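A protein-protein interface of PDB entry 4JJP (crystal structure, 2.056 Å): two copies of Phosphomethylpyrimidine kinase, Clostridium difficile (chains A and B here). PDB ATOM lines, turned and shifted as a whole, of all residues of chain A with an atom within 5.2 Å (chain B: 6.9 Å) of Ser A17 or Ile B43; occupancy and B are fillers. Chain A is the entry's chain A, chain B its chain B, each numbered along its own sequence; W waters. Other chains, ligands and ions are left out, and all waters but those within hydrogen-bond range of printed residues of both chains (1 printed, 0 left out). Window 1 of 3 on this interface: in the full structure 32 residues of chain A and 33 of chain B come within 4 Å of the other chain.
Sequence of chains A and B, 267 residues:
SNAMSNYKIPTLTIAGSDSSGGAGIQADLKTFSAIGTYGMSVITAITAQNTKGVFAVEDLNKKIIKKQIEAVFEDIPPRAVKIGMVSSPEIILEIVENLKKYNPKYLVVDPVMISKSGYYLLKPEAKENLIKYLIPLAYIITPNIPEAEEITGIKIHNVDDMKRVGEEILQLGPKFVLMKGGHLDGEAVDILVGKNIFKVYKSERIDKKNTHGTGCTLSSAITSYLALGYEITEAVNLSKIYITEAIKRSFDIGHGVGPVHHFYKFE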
ATOM      1  N   ALA A  15      15.959  23.496 -13.113  1.00  0.00           N
ATOM      2  CA  ALA A  15      16.409  24.859 -13.004  1.00  0.00           C
ATOM      3  C   ALA A  15      17.598  24.946 -12.025  1.00  0.00           C
ATOM      4  O   ALA A  15      18.014  23.939 -11.410  1.00  0.00           O
ATOM      5  CB  ALA A  15      15.231  25.751 -12.499  1.00  0.00           C
ATOM      6  N   GLY A  16      18.122  26.151 -11.856  1.00  0.00           N
ATOM      7  CA  GLY A  16      19.249  26.384 -10.927  1.00  0.00           C
ATOM      8  C   GLY A  16      18.815  26.526  -9.472  1.00  0.00           C
ATOM      9  O   GLY A  16      17.648  26.766  -9.167  1.00  0.00           O
ATOM     10  N   SER A  17      19.756  26.347  -8.559  1.00  0.00           N
ATOM     11  CA  SER A  17      19.456  26.511  -7.150  1.00  0.00           C
ATOM     12  C   SER A  17      19.736  27.960  -6.731  1.00  0.00           C
ATOM     13  O   SER A  17      20.741  28.530  -7.104  1.00  0.00           O
ATOM     14  CB  SER A  17      20.323  25.571  -6.330  1.00  0.00           C
ATOM     15  OG  SER A  17      20.236  25.897  -4.955  1.00  0.00           O
ATOM     16  N   ASP A  18      18.836  28.533  -5.937  1.00  0.00           N
ATOM     17  CA  ASP A  18      18.996  29.864  -5.364  1.00  0.00           C
ATOM     18  C   ASP A  18      18.995  29.726  -3.824  1.00  0.00           C
ATOM     19  O   ASP A  18      17.952  29.489  -3.210  1.00  0.00           O
ATOM     20  CB  ASP A  18      17.859  30.759  -5.850  1.00  0.00           C
ATOM     21  CG  ASP A  18      17.689  32.024  -5.008  1.00  0.00           C
ATOM     22  OD1 ASP A  18      18.597  32.410  -4.239  1.00  0.00           O
ATOM     23  OD2 ASP A  18      16.609  32.629  -5.107  1.00  0.00           O
ATOM     24  N   SER A  19      20.181  29.881  -3.223  1.00  0.00           N
ATOM     25  CA  SER A  19      20.371  29.755  -1.773  1.00  0.00           C
ATOM     26  C   SER A  19      19.351  30.516  -0.891  1.00  0.00           C
ATOM     27  O   SER A  19      18.883  29.985   0.116  1.00  0.00           O
ATOM     28  CB  SER A  19      21.813  30.158  -1.392  1.00  0.00           C
ATOM     29  OG  SER A  19      22.065  31.528  -1.656  1.00  0.00           O
ATOM     30  N   ILE A  25      14.739  26.414  -8.171  1.00  0.00           N
ATOM     31  CA  ILE A  25      14.069  25.206  -7.666  1.00  0.00           C
ATOM     32  C   ILE A  25      13.447  25.379  -6.285  1.00  0.00           C
ATOM     33  O   ILE A  25      12.418  24.761  -5.966  1.00  0.00           O
ATOM     34  CB  ILE A  25      14.984  23.960  -7.785  1.00  0.00           C
ATOM     35  CG1 ILE A  25      16.165  23.970  -6.796  1.00  0.00           C
ATOM     36  CG2 ILE A  25      15.481  23.864  -9.230  1.00  0.00           C
ATOM     37  CD1 ILE A  25      15.960  23.212  -5.526  1.00  0.00           C
ATOM     38  N   GLN A  26      14.036  26.246  -5.482  1.00  0.00           N
ATOM     39  CA  GLN A  26      13.512  26.481  -4.144  1.00  0.00           C
ATOM     40  C   GLN A  26      12.096  27.056  -4.228  1.00  0.00           C
ATOM     41  O   GLN A  26      11.204  26.565  -3.586  1.00  0.00           O
ATOM     42  CB  GLN A  26      14.446  27.393  -3.323  1.00  0.00           C
ATOM     43  CG  GLN A  26      15.783  26.749  -2.885  1.00  0.00           C
ATOM     44  CD  GLN A  26      16.830  26.580  -3.973  1.00  0.00           C
ATOM     45  OE1 GLN A  26      16.701  27.085  -5.095  1.00  0.00           O
ATOM     46  NE2 GLN A  26      17.901  25.884  -3.628  1.00  0.00           N
ATOM     47  N   ILE A  43      18.802  19.895 -10.716  1.00  0.00           N
ATOM     48  CA  ILE A  43      19.515  21.143 -10.502  1.00  0.00           C
ATOM     49  C   ILE A  43      20.536  21.322 -11.617  1.00  0.00           C
ATOM     50  O   ILE A  43      21.321  20.409 -11.894  1.00  0.00           O
ATOM     51  CB  ILE A  43      20.285  21.172  -9.165  1.00  0.00           C
ATOM     52  CG1 ILE A  43      19.399  20.838  -7.960  1.00  0.00           C
ATOM     53  CG2 ILE A  43      21.014  22.526  -9.004  1.00  0.00           C
ATOM     54  CD1 ILE A  43      18.217  21.654  -7.843  1.00  0.00           C
ATOM     55  N   ALA A  45      22.466  24.430 -11.869  1.00  0.00           N
ATOM     56  CA  ALA A  45      23.467  25.389 -11.474  1.00  0.00           C
ATOM     57  C   ALA A  45      23.278  25.741 -10.018  1.00  0.00           C
ATOM     58  O   ALA A  45      22.200  25.538  -9.460  1.00  0.00           O
ATOM     59  CB  ALA A  45      23.354  26.652 -12.360  1.00  0.00           C
ATOM     60  N   ILE A  46      24.343  26.259  -9.401  1.00  0.00           N
ATOM     61  CA  ILE A  46      24.322  26.639  -7.998  1.00  0.00           C
ATOM     62  C   ILE A  46      24.608  28.111  -7.901  1.00  0.00           C
ATOM     63  O   ILE A  46      25.649  28.582  -8.395  1.00  0.00           O
ATOM     64  CB  ILE A  46      25.408  25.905  -7.194  1.00  0.00           C
ATOM     65  CG1 ILE A  46      25.235  24.390  -7.333  1.00  0.00           C
ATOM     66  CG2 ILE A  46      25.353  26.334  -5.733  1.00  0.00           C
ATOM     67  CD1 ILE A  46      23.926  23.871  -6.764  1.00  0.00           C
ATOM     68  N   THR A  47      23.689  28.830  -7.263  1.00  0.00           N
ATOM     69  CA  THR A  47      23.798  30.269  -7.099  1.00  0.00           C
ATOM     70  C   THR A  47      23.730  30.660  -5.630  1.00  0.00           C
ATOM     71  O   THR A  47      22.822  30.223  -4.895  1.00  0.00           O
ATOM     72  CB  THR A  47      22.661  31.024  -7.834  1.00  0.00           C
ATOM     73  OG1 THR A  47      22.856  30.933  -9.249  1.00  0.00           O
ATOM     74  CG2 THR A  47      22.682  32.505  -7.460  1.00  0.00           C
ATOM     75  N   THR B  13      18.347  24.713   5.503  1.00  0.00           N
ATOM     76  CA  THR B  13      18.804  23.338   5.441  1.00  0.00           C
ATOM     77  C   THR B  13      20.177  23.343   4.779  1.00  0.00           C
ATOM     78  O   THR B  13      20.407  24.039   3.784  1.00  0.00           O
ATOM     79  CB  THR B  13      17.878  22.387   4.656  1.00  0.00           C
ATOM     80  OG1 THR B  13      18.490  21.086   4.613  1.00  0.00           O
ATOM     81  CG2 THR B  13      17.625  22.846   3.199  1.00  0.00           C
ATOM     82  N   ILE B  14      21.093  22.573   5.348  1.00  0.00           N
ATOM     83  CA  ILE B  14      22.419  22.385   4.792  1.00  0.00           C
ATOM     84  C   ILE B  14      22.549  20.877   4.592  1.00  0.00           C
ATOM     85  O   ILE B  14      22.667  20.129   5.562  1.00  0.00           O
ATOM     86  CB  ILE B  14      23.557  22.893   5.710  1.00  0.00           C
ATOM     87  CG1 ILE B  14      23.392  24.376   6.050  1.00  0.00           C
ATOM     88  CG2 ILE B  14      24.886  22.690   5.023  1.00  0.00           C
ATOM     89  CD1 ILE B  14      24.457  24.924   7.004  1.00  0.00           C
ATOM     90  N   ALA B  15      22.505  20.448   3.334  1.00  0.00           N
ATOM     91  CA  ALA B  15      22.556  19.036   2.973  1.00  0.00           C
ATOM     92  C   ALA B  15      22.781  18.868   1.467  1.00  0.00           C
ATOM     93  O   ALA B  15      22.904  19.841   0.726  1.00  0.00           O
ATOM     94  CB  ALA B  15      21.237  18.323   3.405  1.00  0.00           C
ATOM     95  N   GLY B  16      22.837  17.625   1.023  1.00  0.00           N
ATOM     96  CA  GLY B  16      22.996  17.326  -0.391  1.00  0.00           C
ATOM     97  C   GLY B  16      21.680  17.422  -1.137  1.00  0.00           C
ATOM     98  O   GLY B  16      20.611  17.468  -0.529  1.00  0.00           O
ATOM     99  N   SER B  17      21.769  17.453  -2.465  1.00  0.00           N
ATOM    100  CA  SER B  17      20.586  17.489  -3.317  1.00  0.00           C
ATOM    101  C   SER B  17      20.215  16.069  -3.789  1.00  0.00           C
ATOM    102  O   SER B  17      21.075  15.342  -4.277  1.00  0.00           O
ATOM    103  CB  SER B  17      20.862  18.401  -4.529  1.00  0.00           C
ATOM    104  OG  SER B  17      19.763  18.427  -5.418  1.00  0.00           O
ATOM    105  N   ILE B  25      17.943  18.305   0.628  1.00  0.00           N
ATOM    106  CA  ILE B  25      17.401  19.660   0.728  1.00  0.00           C
ATOM    107  C   ILE B  25      15.970  19.756   0.182  1.00  0.00           C
ATOM    108  O   ILE B  25      15.180  20.558   0.686  1.00  0.00           O
ATOM    109  CB  ILE B  25      18.352  20.743   0.092  1.00  0.00           C
ATOM    110  CG1 ILE B  25      18.467  20.601  -1.435  1.00  0.00           C
ATOM    111  CG2 ILE B  25      19.724  20.730   0.757  1.00  0.00           C
ATOM    112  CD1 ILE B  25      17.462  21.388  -2.203  1.00  0.00           C
ATOM    113  N   GLN B  26      15.636  18.902  -0.801  1.00  0.00           N
ATOM    114  CA  GLN B  26      14.291  18.890  -1.414  1.00  0.00           C
ATOM    115  C   GLN B  26      13.232  18.535  -0.396  1.00  0.00           C
ATOM    116  O   GLN B  26      12.228  19.221  -0.272  1.00  0.00           O
ATOM    117  CB  GLN B  26      14.191  17.894  -2.583  1.00  0.00           C
ATOM    118  CG  GLN B  26      14.884  18.306  -3.854  1.00  0.00           C
ATOM    119  CD  GLN B  26      16.382  18.209  -3.828  1.00  0.00           C
ATOM    120  OE1 GLN B  26      16.983  17.695  -2.890  1.00  0.00           O
ATOM    121  NE2 GLN B  26      17.005  18.698  -4.884  1.00  0.00           N
ATOM    122  N   LEU B  29      12.993  21.422   2.248  1.00  0.00           N
ATOM    123  CA  LEU B  29      12.294  22.608   1.743  1.00  0.00           C
ATOM    124  C   LEU B  29      10.787  22.384   1.621  1.00  0.00           C
ATOM    125  O   LEU B  29      10.000  23.288   1.911  1.00  0.00           O
ATOM    126  CB  LEU B  29      12.864  23.047   0.383  1.00  0.00           C
ATOM    127  CG  LEU B  29      14.293  23.602   0.363  1.00  0.00           C
ATOM    128  CD1 LEU B  29      14.809  23.794  -1.068  1.00  0.00           C
ATOM    129  CD2 LEU B  29      14.360  24.907   1.177  1.00  0.00           C
ATOM    130  N   SER B  41      18.543  27.232   1.505  1.00  0.00           N
ATOM    131  CA  SER B  41      19.389  26.054   1.392  1.00  0.00           C
ATOM    132  C   SER B  41      20.811  26.274   0.924  1.00  0.00           C
ATOM    133  O   SER B  41      21.100  27.099   0.053  1.00  0.00           O
ATOM    134  CB  SER B  41      18.739  25.021   0.459  1.00  0.00           C
ATOM    135  OG  SER B  41      18.770  25.456  -0.895  1.00  0.00           O
ATOM    136  N   VAL B  42      21.698  25.538   1.564  1.00  0.00           N
ATOM    137  CA  VAL B  42      23.066  25.454   1.166  1.00  0.00           C
ATOM    138  C   VAL B  42      23.201  24.009   0.692  1.00  0.00           C
ATOM    139  O   VAL B  42      23.087  23.074   1.476  1.00  0.00           O
ATOM    140  CB  VAL B  42      24.020  25.701   2.317  1.00  0.00           C
ATOM    141  CG1 VAL B  42      25.450  25.468   1.856  1.00  0.00           C
ATOM    142  CG2 VAL B  42      23.840  27.116   2.863  1.00  0.00           C
ATOM    143  N   ILE B  43      23.427  23.842  -0.603  1.00  0.00           N
ATOM    144  CA  ILE B  43      23.636  22.535  -1.228  1.00  0.00           C
ATOM    145  C   ILE B  43      25.117  22.173  -1.144  1.00  0.00           C
ATOM    146  O   ILE B  43      25.978  22.982  -1.485  1.00  0.00           O
ATOM    147  CB  ILE B  43      23.121  22.544  -2.694  1.00  0.00           C
ATOM    148  CG1 ILE B  43      21.613  22.869  -2.684  1.00  0.00           C
ATOM    149  CG2 ILE B  43      23.416  21.200  -3.381  1.00  0.00           C
ATOM    150  CD1 ILE B  43      20.909  22.666  -4.026  1.00  0.00           C
ATOM    151  N   THR B  44      25.400  20.953  -0.682  1.00  0.00           N
ATOM    152  CA  THR B  44      26.755  20.459  -0.477  1.00  0.00           C
ATOM    153  C   THR B  44      27.170  19.403  -1.481  1.00  0.00           C
ATOM    154  O   THR B  44      28.366  19.143  -1.672  1.00  0.00           O
ATOM    155  CB  THR B  44      26.936  19.903   0.974  1.00  0.00           C
ATOM    156  OG1 THR B  44      25.925  18.937   1.271  1.00  0.00           O
ATOM    157  CG2 THR B  44      26.851  21.045   2.019  1.00  0.00           C
ATOM    158  N   ALA B  45      26.198  18.811  -2.152  1.00  0.00           N
ATOM    159  CA  ALA B  45      26.495  17.746  -3.085  1.00  0.00           C
ATOM    160  C   ALA B  45      25.272  17.516  -3.941  1.00  0.00           C
ATOM    161  O   ALA B  45      24.167  17.856  -3.542  1.00  0.00           O
ATOM    162  CB  ALA B  45      26.858  16.452  -2.327  1.00  0.00           C
ATOM    163  N   ILE B  46      25.480  16.939  -5.120  1.00  0.00           N
ATOM    164  CA  ILE B  46      24.391  16.664  -6.060  1.00  0.00           C
ATOM    165  C   ILE B  46      24.297  15.154  -6.234  1.00  0.00           C
ATOM    166  O   ILE B  46      25.299  14.514  -6.586  1.00  0.00           O
ATOM    167  CB  ILE B  46      24.697  17.310  -7.437  1.00  0.00           C
ATOM    168  CG1 ILE B  46      24.853  18.834  -7.311  1.00  0.00           C
ATOM    169  CG2 ILE B  46      23.618  16.956  -8.450  1.00  0.00           C
ATOM    170  CD1 ILE B  46      23.598  19.567  -6.896  1.00  0.00           C
ATOM    171  N   LEU B  60      29.981  19.251  -4.127  1.00  0.00           N
ATOM    172  CA  LEU B  60      30.291  20.572  -4.685  1.00  0.00           C
ATOM    173  C   LEU B  60      31.601  21.047  -4.072  1.00  0.00           C
ATOM    174  O   LEU B  60      32.014  20.573  -3.022  1.00  0.00           O
ATOM    175  CB  LEU B  60      29.196  21.592  -4.409  1.00  0.00           C
ATOM    176  CG  LEU B  60      27.857  21.270  -5.061  1.00  0.00           C
ATOM    177  CD1 LEU B  60      26.780  22.291  -4.643  1.00  0.00           C
ATOM    178  CD2 LEU B  60      28.032  21.205  -6.594  1.00  0.00           C
ATOM    179  N   ASN B  61      32.249  21.980  -4.749  1.00  0.00           N
ATOM    180  CA  ASN B  61      33.505  22.525  -4.278  1.00  0.00           C
ATOM    181  C   ASN B  61      33.262  23.415  -3.048  1.00  0.00           C
ATOM    182  O   ASN B  61      32.181  23.969  -2.857  1.00  0.00           O
ATOM    183  CB  ASN B  61      34.247  23.258  -5.403  1.00  0.00           C
ATOM    184  CG  ASN B  61      33.645  24.599  -5.721  1.00  0.00           C
ATOM    185  OD1 ASN B  61      33.759  25.553  -4.942  1.00  0.00           O
ATOM    186  ND2 ASN B  61      33.032  24.701  -6.893  1.00  0.00           N
ATOM    187  N   ILE B  64      32.054  27.372  -3.407  1.00  0.00           N
ATOM    188  CA  ILE B  64      30.641  27.629  -3.714  1.00  0.00           C
ATOM    189  C   ILE B  64      29.798  27.317  -2.490  1.00  0.00           C
ATOM    190  O   ILE B  64      28.794  27.969  -2.250  1.00  0.00           O
ATOM    191  CB  ILE B  64      30.094  26.881  -4.951  1.00  0.00           C
ATOM    192  CG1 ILE B  64      28.741  27.506  -5.360  1.00  0.00           C
ATOM    193  CG2 ILE B  64      29.932  25.376  -4.684  1.00  0.00           C
ATOM    194  CD1 ILE B  64      28.808  28.982  -5.767  1.00  0.00           C
ATOM    195  N   ILE B  65      30.216  26.343  -1.693  1.00  0.00           N
ATOM    196  CA  ILE B  65      29.482  26.037  -0.458  1.00  0.00           C
ATOM    197  C   ILE B  65      29.618  27.231   0.518  1.00  0.00           C
ATOM    198  O   ILE B  65      28.644  27.657   1.154  1.00  0.00           O
ATOM    199  CB  ILE B  65      29.980  24.708   0.173  1.00  0.00           C
ATOM    200  CG1 ILE B  65      29.553  23.522  -0.706  1.00  0.00           C
ATOM    201  CG2 ILE B  65      29.445  24.529   1.594  1.00  0.00           C
ATOM    202  CD1 ILE B  65      30.138  22.167  -0.246  1.00  0.00           C
ATOM    203  N   GLN B  68      27.373  30.196  -0.556  1.00  0.00           N
ATOM    204  CA  GLN B  68      25.977  29.948  -0.212  1.00  0.00           C
ATOM    205  C   GLN B  68      25.744  30.258   1.264  1.00  0.00           C
ATOM    206  O   GLN B  68      24.763  30.909   1.621  1.00  0.00           O
ATOM    207  CB  GLN B  68      25.609  28.500  -0.515  1.00  0.00           C
ATOM    208  CG  GLN B  68      25.595  28.125  -1.985  1.00  0.00           C
ATOM    209  CD  GLN B  68      25.323  26.646  -2.189  1.00  0.00           C
ATOM    210  OE1 GLN B  68      24.171  26.240  -2.318  1.00  0.00           O
ATOM    211  NE2 GLN B  68      26.372  25.825  -2.151  1.00  0.00           N
HETATM  212  O   HOH W   1      22.149  27.465  -4.095  1.00  0.00           O
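The side-chain hydroxyl (OG) of Ser A17 is in hydrogen-bond range of the side-chain amide nitrogen (NE2) of Gln A26 (2.7 Å).
The backbone NH (N) of Ser A17 lies within hydrogen-bond range of the backbone carbonyl oxygen (O) of Ala A45, 2.7 Å away.
The side-chain amide oxygen of Gln A26 lies within hydrogen-bond range of the backbone NH of Asp A18 (2.7 Å).
The backbone NH (N) of Ser A19 sits at hydrogen-bond distance from the backbone carbonyl oxygen (O) of Thr A47 (3.1 Å).
The side-chain hydroxyl (OG) of Ser B17 lies within hydrogen-bond range of the side-chain amide nitrogen (NE2) of Gln B26 (2.8 Å).
The side-chain amide nitrogen (NE2) of Gln B68 sits close to the backbone carbonyl oxygen (O) of Ile B64 (3.2 Å).
O of Ser A19 lies within hydrogen-bond range of N of Ser B41, at 3.1 Å.
The side-chain amide nitrogen of Gln A26 lies within hydrogen-bond range of the side-chain hydroxyl of Ser B41, 2.9 Å away.
Water W1 lies within hydrogen-bond range of the side-chain hydroxyl (OG) of Ser A17 (2.6 Å), the backbone carbonyl oxygen (O) of Thr A47 (2.9 Å), the side-chain amide oxygen (OE1) of Gln B68 (3.0 Å) and the backbone NH (N) of Ser A19 (3.2 Å).
Of the printed residues of chain B, Ser A17 touches Ile B43.
Of the printed residues of chain B, Ile A46 touches Leu B60 (3.7 Å), Ile B64 (3.6 Å) and Gln B68 (3.6 Å).
Printed residues of chain A within 4 Å of Ser B41: Ser A19 and Gln A26.
Ile B43 touches just one residue of chain A: Ser A17.
Ile B46 touches none of the printed residues of chain A.
Of the printed residues of chain A, Leu B60 touches Ile A46.
Asn B61 touches none of the printed residues of chain A.
The nearest residue of chain B that does not touch Ser A17 is Ser B41 (4.3 Å).
The nearest residue of chain A that does not touch Ile B43 is Ile A46 (4.2 Å).
The nearest printed residue of chain A that does not touch Ile B64 is Thr A47 (5.3 Å).
Among the printed residues, merely in contact across the chains: Ser A17 with Ile B43, Gln A26 with Leu B29, Ile A43 with Ser B17, Ile A46 with Leu B60, Ile A46 with Ile B64 and Ile A46 with Gln B68.
Ser A17 touches Ile B43, and with the chains exchanged Ile A43 touches Ser B17.
Of the 8 pairs that touch across the chains among the printed residues, 2 have their exchanged pair printed and touching as well.
Of the 19 printed residues of chain B, 7 touch a printed residue of chain A.
Printed residues of chain B that touch a printed residue of chain A: Ser B17, Leu B29, Ser B41, Ile B43, Leu B60, Ile B64 and Gln B68.
Hydrophobic or aromatic side chains of chain B within 4 Å of the printed part of chain A: Leu B29, Ile B43, Leu B60 and Ile B64.
Printed residues of chain A that touch a printed residue of chain B: Ser A17, Ser A19, Gln A26, Ile A43 and Ile A46.
Hydrophobic or aromatic side chains of chain A that line the printed part of chain B: Ile A43 and Ile A46.
Along chain A the printed residues that touch a printed residue of chain B span positions 17 to 46.
Among the printed residues, no Asp or Glu carboxylate lies within 4 Å of a Lys or Arg side-chain nitrogen of the other chain.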
